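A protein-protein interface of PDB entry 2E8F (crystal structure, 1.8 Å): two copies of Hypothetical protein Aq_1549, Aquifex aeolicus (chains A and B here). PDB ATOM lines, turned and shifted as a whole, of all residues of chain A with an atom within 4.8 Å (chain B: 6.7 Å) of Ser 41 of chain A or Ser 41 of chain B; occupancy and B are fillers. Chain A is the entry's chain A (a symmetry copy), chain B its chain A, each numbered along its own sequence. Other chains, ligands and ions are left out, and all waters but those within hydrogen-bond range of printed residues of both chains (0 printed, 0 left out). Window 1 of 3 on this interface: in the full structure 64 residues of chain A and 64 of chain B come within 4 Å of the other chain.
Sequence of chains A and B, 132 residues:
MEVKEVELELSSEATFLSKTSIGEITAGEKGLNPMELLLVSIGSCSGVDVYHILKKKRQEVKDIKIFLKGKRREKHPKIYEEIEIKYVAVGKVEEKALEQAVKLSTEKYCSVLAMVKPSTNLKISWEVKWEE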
ATOM      1  N   PRO A  34      -7.496  22.150  13.545  1.00  0.00           N
ATOM      2  CA  PRO A  34      -7.121  22.255  12.128  1.00  0.00           C
ATOM      3  C   PRO A  34      -8.222  22.716  11.171  1.00  0.00           C
ATOM      4  O   PRO A  34      -7.976  23.557  10.301  1.00  0.00           O
ATOM      5  CB  PRO A  34      -6.601  20.855  11.806  1.00  0.00           C
ATOM      6  CG  PRO A  34      -5.986  20.434  13.118  1.00  0.00           C
ATOM      7  CD  PRO A  34      -7.048  20.865  14.109  1.00  0.00           C
ATOM      8  N   LEU A  37      -8.874  26.246  11.630  1.00  0.00           N
ATOM      9  CA  LEU A  37      -7.766  26.986  11.031  1.00  0.00           C
ATOM     10  C   LEU A  37      -7.947  27.114   9.522  1.00  0.00           C
ATOM     11  O   LEU A  37      -7.508  28.095   8.925  1.00  0.00           O
ATOM     12  CB  LEU A  37      -6.417  26.322  11.347  1.00  0.00           C
ATOM     13  CG  LEU A  37      -5.825  26.696  12.704  1.00  0.00           C
ATOM     14  CD1 LEU A  37      -4.494  25.980  12.903  1.00  0.00           C
ATOM     15  CD2 LEU A  37      -5.621  28.211  12.765  1.00  0.00           C
ATOM     16  N   LEU A  38      -8.587  26.129   8.896  1.00  0.00           N
ATOM     17  CA  LEU A  38      -8.822  26.229   7.460  1.00  0.00           C
ATOM     18  C   LEU A  38      -9.756  27.411   7.222  1.00  0.00           C
ATOM     19  O   LEU A  38      -9.548  28.208   6.304  1.00  0.00           O
ATOM     20  CB  LEU A  38      -9.461  24.946   6.913  1.00  0.00           C
ATOM     21  CG  LEU A  38      -9.945  25.023   5.456  1.00  0.00           C
ATOM     22  CD1 LEU A  38      -8.776  25.355   4.543  1.00  0.00           C
ATOM     23  CD2 LEU A  38     -10.580  23.704   5.052  1.00  0.00           C
ATOM     24  N   LEU A  39     -10.792  27.525   8.050  1.00  0.00           N
ATOM     25  CA  LEU A  39     -11.731  28.632   7.898  1.00  0.00           C
ATOM     26  C   LEU A  39     -11.012  29.959   8.142  1.00  0.00           C
ATOM     27  O   LEU A  39     -11.317  30.958   7.493  1.00  0.00           O
ATOM     28  CB  LEU A  39     -12.907  28.486   8.867  1.00  0.00           C
ATOM     29  CG  LEU A  39     -13.847  27.310   8.592  1.00  0.00           C
ATOM     30  CD1 LEU A  39     -14.948  27.314   9.639  1.00  0.00           C
ATOM     31  CD2 LEU A  39     -14.449  27.422   7.185  1.00  0.00           C
ATOM     32  N   VAL A  40     -10.062  29.977   9.073  1.00  0.00           N
ATOM     33  CA  VAL A  40      -9.320  31.204   9.335  1.00  0.00           C
ATOM     34  C   VAL A  40      -8.458  31.541   8.116  1.00  0.00           C
ATOM     35  O   VAL A  40      -8.329  32.714   7.750  1.00  0.00           O
ATOM     36  CB  VAL A  40      -8.400  31.087  10.596  1.00  0.00           C
ATOM     37  CG1 VAL A  40      -7.467  32.291  10.688  1.00  0.00           C
ATOM     38  CG2 VAL A  40      -9.247  30.994  11.858  1.00  0.00           C
ATOM     39  N   SER A  41      -7.884  30.519   7.482  1.00  0.00           N
ATOM     40  CA  SER A  41      -7.037  30.731   6.303  1.00  0.00           C
ATOM     41  C   SER A  41      -7.861  31.343   5.183  1.00  0.00           C
ATOM     42  O   SER A  41      -7.444  32.308   4.541  1.00  0.00           O
ATOM     43  CB  SER A  41      -6.437  29.407   5.827  1.00  0.00           C
ATOM     44  OG  SER A  41      -5.620  28.844   6.837  1.00  0.00           O
ATOM     45  N   ILE A  42      -9.035  30.770   4.956  1.00  0.00           N
ATOM     46  CA  ILE A  42      -9.949  31.252   3.924  1.00  0.00           C
ATOM     47  C   ILE A  42     -10.381  32.687   4.230  1.00  0.00           C
ATOM     48  O   ILE A  42     -10.284  33.578   3.379  1.00  0.00           O
ATOM     49  CB  ILE A  42     -11.216  30.361   3.859  1.00  0.00           C
ATOM     50  CG1 ILE A  42     -10.850  28.958   3.355  1.00  0.00           C
ATOM     51  CG2 ILE A  42     -12.256  30.996   2.963  1.00  0.00           C
ATOM     52  CD1 ILE A  42     -11.984  27.943   3.494  1.00  0.00           C
ATOM     53  N   GLY A  43     -10.868  32.897   5.450  1.00  0.00           N
ATOM     54  CA  GLY A  43     -11.324  34.215   5.850  1.00  0.00           C
ATOM     55  C   GLY A  43     -10.268  35.301   5.767  1.00  0.00           C
ATOM     56  O   GLY A  43     -10.534  36.387   5.247  1.00  0.00           O
ATOM     57  N   SER A  44      -9.067  35.021   6.267  1.00  0.00           N
ATOM     58  CA  SER A  44      -8.001  36.021   6.234  1.00  0.00           C
ATOM     59  C   SER A  44      -7.491  36.282   4.817  1.00  0.00           C
ATOM     60  O   SER A  44      -7.224  37.431   4.449  1.00  0.00           O
ATOM     61  CB  SER A  44      -6.841  35.606   7.157  1.00  0.00           C
ATOM     62  OG  SER A  44      -6.298  34.344   6.789  1.00  0.00           O
ATOM     63  N   CYS A  45      -7.357  35.229   4.016  1.00  0.00           N
ATOM     64  CA  CYS A  45      -6.882  35.404   2.648  1.00  0.00           C
ATOM     65  C   CYS A  45      -7.836  36.332   1.895  1.00  0.00           C
ATOM     66  O   CYS A  45      -7.409  37.283   1.231  1.00  0.00           O
ATOM     67  CB  CYS A  45      -6.805  34.057   1.931  1.00  0.00           C
ATOM     68  SG  CYS A  45      -6.089  34.153   0.282  1.00  0.00           S
ATOM     69  N   VAL A 112      -6.558  30.722  -1.219  1.00  0.00           N
ATOM     70  CA  VAL A 112      -7.007  29.657  -0.325  1.00  0.00           C
ATOM     71  C   VAL A 112      -8.390  29.166  -0.749  1.00  0.00           C
ATOM     72  O   VAL A 112      -8.615  27.964  -0.894  1.00  0.00           O
ATOM     73  CB  VAL A 112      -7.062  30.142   1.152  1.00  0.00           C
ATOM     74  CG1 VAL A 112      -7.529  29.001   2.064  1.00  0.00           C
ATOM     75  CG2 VAL A 112      -5.683  30.639   1.590  1.00  0.00           C
ATOM     76  N   LEU B   8     -13.675  36.755  12.248  1.00  0.00           N
ATOM     77  CA  LEU B   8     -12.520  37.621  12.068  1.00  0.00           C
ATOM     78  C   LEU B   8     -12.911  39.085  12.153  1.00  0.00           C
ATOM     79  O   LEU B   8     -14.031  39.459  11.810  1.00  0.00           O
ATOM     80  CB  LEU B   8     -11.865  37.380  10.704  1.00  0.00           C
ATOM     81  CG  LEU B   8     -11.014  36.125  10.487  1.00  0.00           C
ATOM     82  CD1 LEU B   8     -11.824  34.876  10.759  1.00  0.00           C
ATOM     83  CD2 LEU B   8     -10.492  36.130   9.064  1.00  0.00           C
ATOM     84  N   ALA B  27      -4.141  36.929  11.598  1.00  0.00           N
ATOM     85  CA  ALA B  27      -3.852  36.371  10.287  1.00  0.00           C
ATOM     86  C   ALA B  27      -3.995  37.453   9.224  1.00  0.00           C
ATOM     87  O   ALA B  27      -4.980  38.193   9.209  1.00  0.00           O
ATOM     88  CB  ALA B  27      -4.811  35.221   9.994  1.00  0.00           C
ATOM     89  N   ASN B  33       0.655  34.534   7.707  1.00  0.00           N
ATOM     90  CA  ASN B  33       0.330  34.526   6.284  1.00  0.00           C
ATOM     91  C   ASN B  33      -0.778  33.504   6.021  1.00  0.00           C
ATOM     92  O   ASN B  33      -0.649  32.338   6.389  1.00  0.00           O
ATOM     93  CB  ASN B  33       1.577  34.180   5.469  1.00  0.00           C
ATOM     94  CG  ASN B  33       1.290  34.087   3.992  1.00  0.00           C
ATOM     95  OD1 ASN B  33       1.140  32.997   3.443  1.00  0.00           O
ATOM     96  ND2 ASN B  33       1.187  35.243   3.338  1.00  0.00           N
ATOM     97  N   PRO B  34      -1.879  33.925   5.374  1.00  0.00           N
ATOM     98  CA  PRO B  34      -2.983  32.995   5.101  1.00  0.00           C
ATOM     99  C   PRO B  34      -2.613  31.706   4.363  1.00  0.00           C
ATOM    100  O   PRO B  34      -3.074  30.624   4.737  1.00  0.00           O
ATOM    101  CB  PRO B  34      -3.976  33.859   4.326  1.00  0.00           C
ATOM    102  CG  PRO B  34      -3.760  35.221   4.940  1.00  0.00           C
ATOM    103  CD  PRO B  34      -2.248  35.299   4.993  1.00  0.00           C
ATOM    104  N   MET B  35      -1.791  31.806   3.325  1.00  0.00           N
ATOM    105  CA  MET B  35      -1.407  30.610   2.584  1.00  0.00           C
ATOM    106  C   MET B  35      -0.473  29.700   3.390  1.00  0.00           C
ATOM    107  O   MET B  35      -0.477  28.479   3.197  1.00  0.00           O
ATOM    108  CB  MET B  35      -0.809  30.992   1.231  1.00  0.00           C
ATOM    109  CG  MET B  35      -1.888  31.279   0.170  1.00  0.00           C
ATOM    110  SD  MET B  35      -2.780  29.819  -0.452  1.00  0.00           S
ATOM    111  CE  MET B  35      -1.731  29.397  -1.823  1.00  0.00           C
ATOM    112  N   GLU B  36       0.327  30.275   4.286  1.00  0.00           N
ATOM    113  CA  GLU B  36       1.170  29.446   5.143  1.00  0.00           C
ATOM    114  C   GLU B  36       0.231  28.763   6.145  1.00  0.00           C
ATOM    115  O   GLU B  36       0.440  27.605   6.523  1.00  0.00           O
ATOM    116  CB  GLU B  36       2.210  30.285   5.895  1.00  0.00           C
ATOM    117  CG  GLU B  36       3.353  30.765   5.022  1.00  0.00           C
ATOM    118  CD  GLU B  36       4.430  31.504   5.802  1.00  0.00           C
ATOM    119  OE1 GLU B  36       4.263  31.706   7.025  1.00  0.00           O
ATOM    120  OE2 GLU B  36       5.442  31.884   5.182  1.00  0.00           O
ATOM    121  N   LEU B  37      -0.810  29.479   6.573  1.00  0.00           N
ATOM    122  CA  LEU B  37      -1.773  28.904   7.509  1.00  0.00           C
ATOM    123  C   LEU B  37      -2.515  27.730   6.878  1.00  0.00           C
ATOM    124  O   LEU B  37      -2.910  26.799   7.574  1.00  0.00           O
ATOM    125  CB  LEU B  37      -2.774  29.961   7.999  1.00  0.00           C
ATOM    126  CG  LEU B  37      -2.278  30.817   9.163  1.00  0.00           C
ATOM    127  CD1 LEU B  37      -3.352  31.824   9.558  1.00  0.00           C
ATOM    128  CD2 LEU B  37      -1.944  29.911  10.349  1.00  0.00           C
ATOM    129  N   LEU B  38      -2.713  27.768   5.562  1.00  0.00           N
ATOM    130  CA  LEU B  38      -3.380  26.648   4.907  1.00  0.00           C
ATOM    131  C   LEU B  38      -2.485  25.421   5.055  1.00  0.00           C
ATOM    132  O   LEU B  38      -2.959  24.324   5.356  1.00  0.00           O
ATOM    133  CB  LEU B  38      -3.618  26.937   3.420  1.00  0.00           C
ATOM    134  CG  LEU B  38      -4.121  25.745   2.591  1.00  0.00           C
ATOM    135  CD1 LEU B  38      -5.439  25.244   3.157  1.00  0.00           C
ATOM    136  CD2 LEU B  38      -4.287  26.158   1.139  1.00  0.00           C
ATOM    137  N   LEU B  39      -1.184  25.606   4.840  1.00  0.00           N
ATOM    138  CA  LEU B  39      -0.255  24.489   4.969  1.00  0.00           C
ATOM    139  C   LEU B  39      -0.246  23.985   6.412  1.00  0.00           C
ATOM    140  O   LEU B  39      -0.119  22.786   6.650  1.00  0.00           O
ATOM    141  CB  LEU B  39       1.158  24.902   4.548  1.00  0.00           C
ATOM    142  CG  LEU B  39       1.338  25.219   3.061  1.00  0.00           C
ATOM    143  CD1 LEU B  39       2.786  25.608   2.820  1.00  0.00           C
ATOM    144  CD2 LEU B  39       0.962  24.001   2.205  1.00  0.00           C
ATOM    145  N   VAL B  40      -0.379  24.892   7.377  1.00  0.00           N
ATOM    146  CA  VAL B  40      -0.405  24.475   8.773  1.00  0.00           C
ATOM    147  C   VAL B  40      -1.680  23.670   9.034  1.00  0.00           C
ATOM    148  O   VAL B  40      -1.650  22.677   9.767  1.00  0.00           O
ATOM    149  CB  VAL B  40      -0.355  25.689   9.759  1.00  0.00           C
ATOM    150  CG1 VAL B  40      -0.632  25.226  11.187  1.00  0.00           C
ATOM    151  CG2 VAL B  40       1.008  26.365   9.692  1.00  0.00           C
ATOM    152  N   SER B  41      -2.791  24.085   8.425  1.00  0.00           N
ATOM    153  CA  SER B  41      -4.067  23.386   8.606  1.00  0.00           C
ATOM    154  C   SER B  41      -3.957  21.968   8.074  1.00  0.00           C
ATOM    155  O   SER B  41      -4.368  21.009   8.729  1.00  0.00           O
ATOM    156  CB  SER B  41      -5.190  24.119   7.870  1.00  0.00           C
ATOM    157  OG  SER B  41      -5.349  25.428   8.387  1.00  0.00           O
ATOM    158  N   ILE B  42      -3.396  21.847   6.878  1.00  0.00           N
ATOM    159  CA  ILE B  42      -3.204  20.548   6.238  1.00  0.00           C
ATOM    160  C   ILE B  42      -2.275  19.675   7.083  1.00  0.00           C
ATOM    161  O   ILE B  42      -2.599  18.528   7.409  1.00  0.00           O
ATOM    162  CB  ILE B  42      -2.571  20.722   4.834  1.00  0.00           C
ATOM    163  CG1 ILE B  42      -3.562  21.419   3.891  1.00  0.00           C
ATOM    164  CG2 ILE B  42      -2.159  19.378   4.277  1.00  0.00           C
ATOM    165  CD1 ILE B  42      -2.940  21.854   2.564  1.00  0.00           C
ATOM    166  N   GLY B  43      -1.114  20.227   7.425  1.00  0.00           N
ATOM    167  CA  GLY B  43      -0.145  19.490   8.214  1.00  0.00           C
ATOM    168  C   GLY B  43      -0.654  19.022   9.564  1.00  0.00           C
ATOM    169  O   GLY B  43      -0.452  17.865   9.937  1.00  0.00           O
ATOM    170  N   SER B  44      -1.322  19.907  10.302  1.00  0.00           N
ATOM    171  CA  SER B  44      -1.833  19.533  11.620  1.00  0.00           C
ATOM    172  C   SER B  44      -2.992  18.540  11.535  1.00  0.00           C
ATOM    173  O   SER B  44      -3.072  17.602  12.336  1.00  0.00           O
ATOM    174  CB  SER B  44      -2.254  20.785  12.411  1.00  0.00           C
ATOM    175  OG  SER B  44      -3.251  21.534  11.726  1.00  0.00           O
ATOM    176  N   CYS B  45      -3.887  18.731  10.571  1.00  0.00           N
ATOM    177  CA  CYS B  45      -5.015  17.818  10.426  1.00  0.00           C
ATOM    178  C   CYS B  45      -4.492  16.402  10.180  1.00  0.00           C
ATOM    179  O   CYS B  45      -4.929  15.440  10.822  1.00  0.00           O
ATOM    180  CB  CYS B  45      -5.904  18.245   9.260  1.00  0.00           C
ATOM    181  SG  CYS B  45      -7.404  17.263   9.093  1.00  0.00           S
ATOM    182  N   SER B  46      -3.542  16.285   9.259  1.00  0.00           N
ATOM    183  CA  SER B  46      -2.964  14.985   8.925  1.00  0.00           C
ATOM    184  C   SER B  46      -2.123  14.473  10.084  1.00  0.00           C
ATOM    185  O   SER B  46      -2.138  13.279  10.400  1.00  0.00           O
ATOM    186  CB  SER B  46      -2.100  15.094   7.665  1.00  0.00           C
ATOM    187  OG  SER B  46      -1.558  13.827   7.313  1.00  0.00           O
ATOM    188  N   GLY B  47      -1.393  15.386  10.723  1.00  0.00           N
ATOM    189  CA  GLY B  47      -0.554  15.016  11.848  1.00  0.00           C
ATOM    190  C   GLY B  47      -1.349  14.365  12.966  1.00  0.00           C
ATOM    191  O   GLY B  47      -0.869  13.436  13.620  1.00  0.00           O
ATOM    192  N   LEU B  68       6.078  20.879   5.045  1.00  0.00           N
ATOM    193  CA  LEU B  68       5.231  21.147   3.892  1.00  0.00           C
ATOM    194  C   LEU B  68       5.791  22.278   3.050  1.00  0.00           C
ATOM    195  O   LEU B  68       6.155  23.331   3.569  1.00  0.00           O
ATOM    196  CB  LEU B  68       3.805  21.496   4.332  1.00  0.00           C
ATOM    197  CG  LEU B  68       3.072  20.421   5.137  1.00  0.00           C
ATOM    198  CD1 LEU B  68       3.219  20.698   6.632  1.00  0.00           C
ATOM    199  CD2 LEU B  68       1.609  20.414   4.740  1.00  0.00           C
ATOM    200  N   CYS B 110      -7.888  12.632   6.618  1.00  0.00           N
ATOM    201  CA  CYS B 110      -7.597  14.065   6.596  1.00  0.00           C
ATOM    202  C   CYS B 110      -8.604  14.930   5.844  1.00  0.00           C
ATOM    203  O   CYS B 110      -8.585  15.003   4.610  1.00  0.00           O
ATOM    204  CB  CYS B 110      -6.202  14.305   6.030  1.00  0.00           C
ATOM    205  SG  CYS B 110      -5.642  15.998   6.324  1.00  0.00           S
ATOM    206  N   VAL B 112      -8.981  18.379   5.851  1.00  0.00           N
ATOM    207  CA  VAL B 112      -8.423  19.568   5.210  1.00  0.00           C
ATOM    208  C   VAL B 112      -7.804  19.195   3.865  1.00  0.00           C
ATOM    209  O   VAL B 112      -8.081  19.829   2.846  1.00  0.00           O
ATOM    210  CB  VAL B 112      -7.344  20.241   6.106  1.00  0.00           C
ATOM    211  CG1 VAL B 112      -6.784  21.487   5.410  1.00  0.00           C
ATOM    212  CG2 VAL B 112      -7.950  20.618   7.459  1.00  0.00           C
ATOM    213  N   LEU B 113      -6.984  18.148   3.860  1.00  0.00           N
ATOM    214  CA  LEU B 113      -6.325  17.704   2.639  1.00  0.00           C
ATOM    215  C   LEU B 113      -7.300  17.260   1.551  1.00  0.00           C
ATOM    216  O   LEU B 113      -7.079  17.531   0.373  1.00  0.00           O
ATOM    217  CB  LEU B 113      -5.354  16.563   2.954  1.00  0.00           C
ATOM    218  CG  LEU B 113      -4.405  16.154   1.828  1.00  0.00           C
ATOM    219  CD1 LEU B 113      -3.688  17.374   1.278  1.00  0.00           C
ATOM    220  CD2 LEU B 113      -3.406  15.140   2.366  1.00  0.00           C
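Among the printed residues, merely in contact across the chains: Pro 34 of chain A with Ser 44 of chain B (3.3 Å), Ser 44 of chain A with Pro 34 of chain B (3.3 Å), Ser 44 of chain A with Leu 8 of chain B (3.3 Å), Gly 43 of chain A with Leu 8 of chain B (3.4 Å), Ser 44 of chain A with Ala 27 of chain B (3.5 Å), Leu 38 of chain A with Leu 38 of chain B (3.6 Å), Val 112 of chain A with Met 35 of chain B (3.6 Å), Pro 34 of chain A with Cys 45 of chain B (3.7 Å), Cys 45 of chain A with Pro 34 of chain B (3.7 Å), Ser 41 of chain A with Pro 34 of chain B (3.7 Å), Pro 34 of chain A with Ser 41 of chain B (3.7 Å) and Ser 41 of chain A with Ser 41 of chain B (3.8 Å).
Of chain B, only Pro 34 (3.7 Å), Leu 37 (3.3 Å), Leu 38 (3.4 Å) and Ser 41 (3.8 Å) come within 4 Å of Ser 41 of chain A.
Printed residues of chain B within 4 Å of Ser 44 of chain A: Leu 8 (3.3 Å), Ala 27 (3.5 Å) and Pro 34 (3.3 Å).
Of the printed residues of chain B, Val 112 of chain A touches Met 35 (3.6 Å).
Of the printed residues of chain A, Ala 27 of chain B touches Ser 44.
Of the printed residues of chain A, Leu 38 of chain B touches Leu 38 (3.6 Å) and Ser 41 (3.4 Å).
Of chain A, only Pro 34, Leu 37, Leu 38 and Ser 41 come within 4 Å of Ser 41 of chain B.
The nearest printed residue of chain A that does not touch Ser 41 of chain B is Leu 39 of chain A (5.8 Å).
Pro 34 of chain A touches Ser 41 of chain B, and with the chains exchanged Ser 41 of chain A touches Pro 34 of chain B.
Pro 34 of chain A touches Ser 44 of chain B, and with the chains exchanged Ser 44 of chain A touches Pro 34 of chain B.
Leu 38 of chain B touches its own counterpart, Leu 38 of chain A.
Ser 41 of chain B touches its own counterpart, Ser 41 of chain A.
Of the 16 pairs that touch across the chains among the printed residues, 12 have their exchanged pair printed and touching as well.
The backbone carbonyl oxygen (O) of Leu 37 of chain B lies within hydrogen-bond range of the side-chain hydroxyl (OG) of Ser 41 of chain B, at 2.9 Å.
O of Ser 41 of chain B lies within hydrogen-bond range of OG of Ser 44 of chain B (3.2 Å).
The side-chain sulfur of Cys 110 of chain B sits at hydrogen-bond distance from the side-chain sulfur of Cys 45 of chain B.
The backbone carbonyl oxygen (O) of Leu 37 of chain A sits at hydrogen-bond distance from the side-chain hydroxyl (OG) of Ser 41 of chain A (2.9 Å).
O of Ser 41 of chain A is in hydrogen-bond range of OG of Ser 44 of chain A (3.2 Å).
The side-chain sulfur of Cys 45 of chain A lies close to the backbone NH of Val 112 of chain A (3.8 Å).
OG of Ser 41 of chain A lies close to O of Leu 37 of chain B (3.5 Å).
The backbone NH (N) of Leu 38 of chain B is in hydrogen-bond range of the side-chain hydroxyl (OG) of Ser 41 of chain A.
The side-chain hydroxyl (OG) of Ser 41 of chain B sits close to the backbone carbonyl oxygen (O) of Leu 37 of chain A, at 3.5 Å.
The side-chain hydroxyl (OG) of Ser 41 of chain B lies within hydrogen-bond range of the backbone NH (N) of Leu 38 of chain A (3.4 Å).
Of the 21 printed residues of chain B, 9 touch a printed residue of chain A.
Of the 11 printed residues of chain A, 8 touch a printed residue of chain B.
Hydrophobic or aromatic side chains of chain A within 4 Å of the printed part of chain B: Pro 34, Leu 37, Leu 38 and Val 112.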
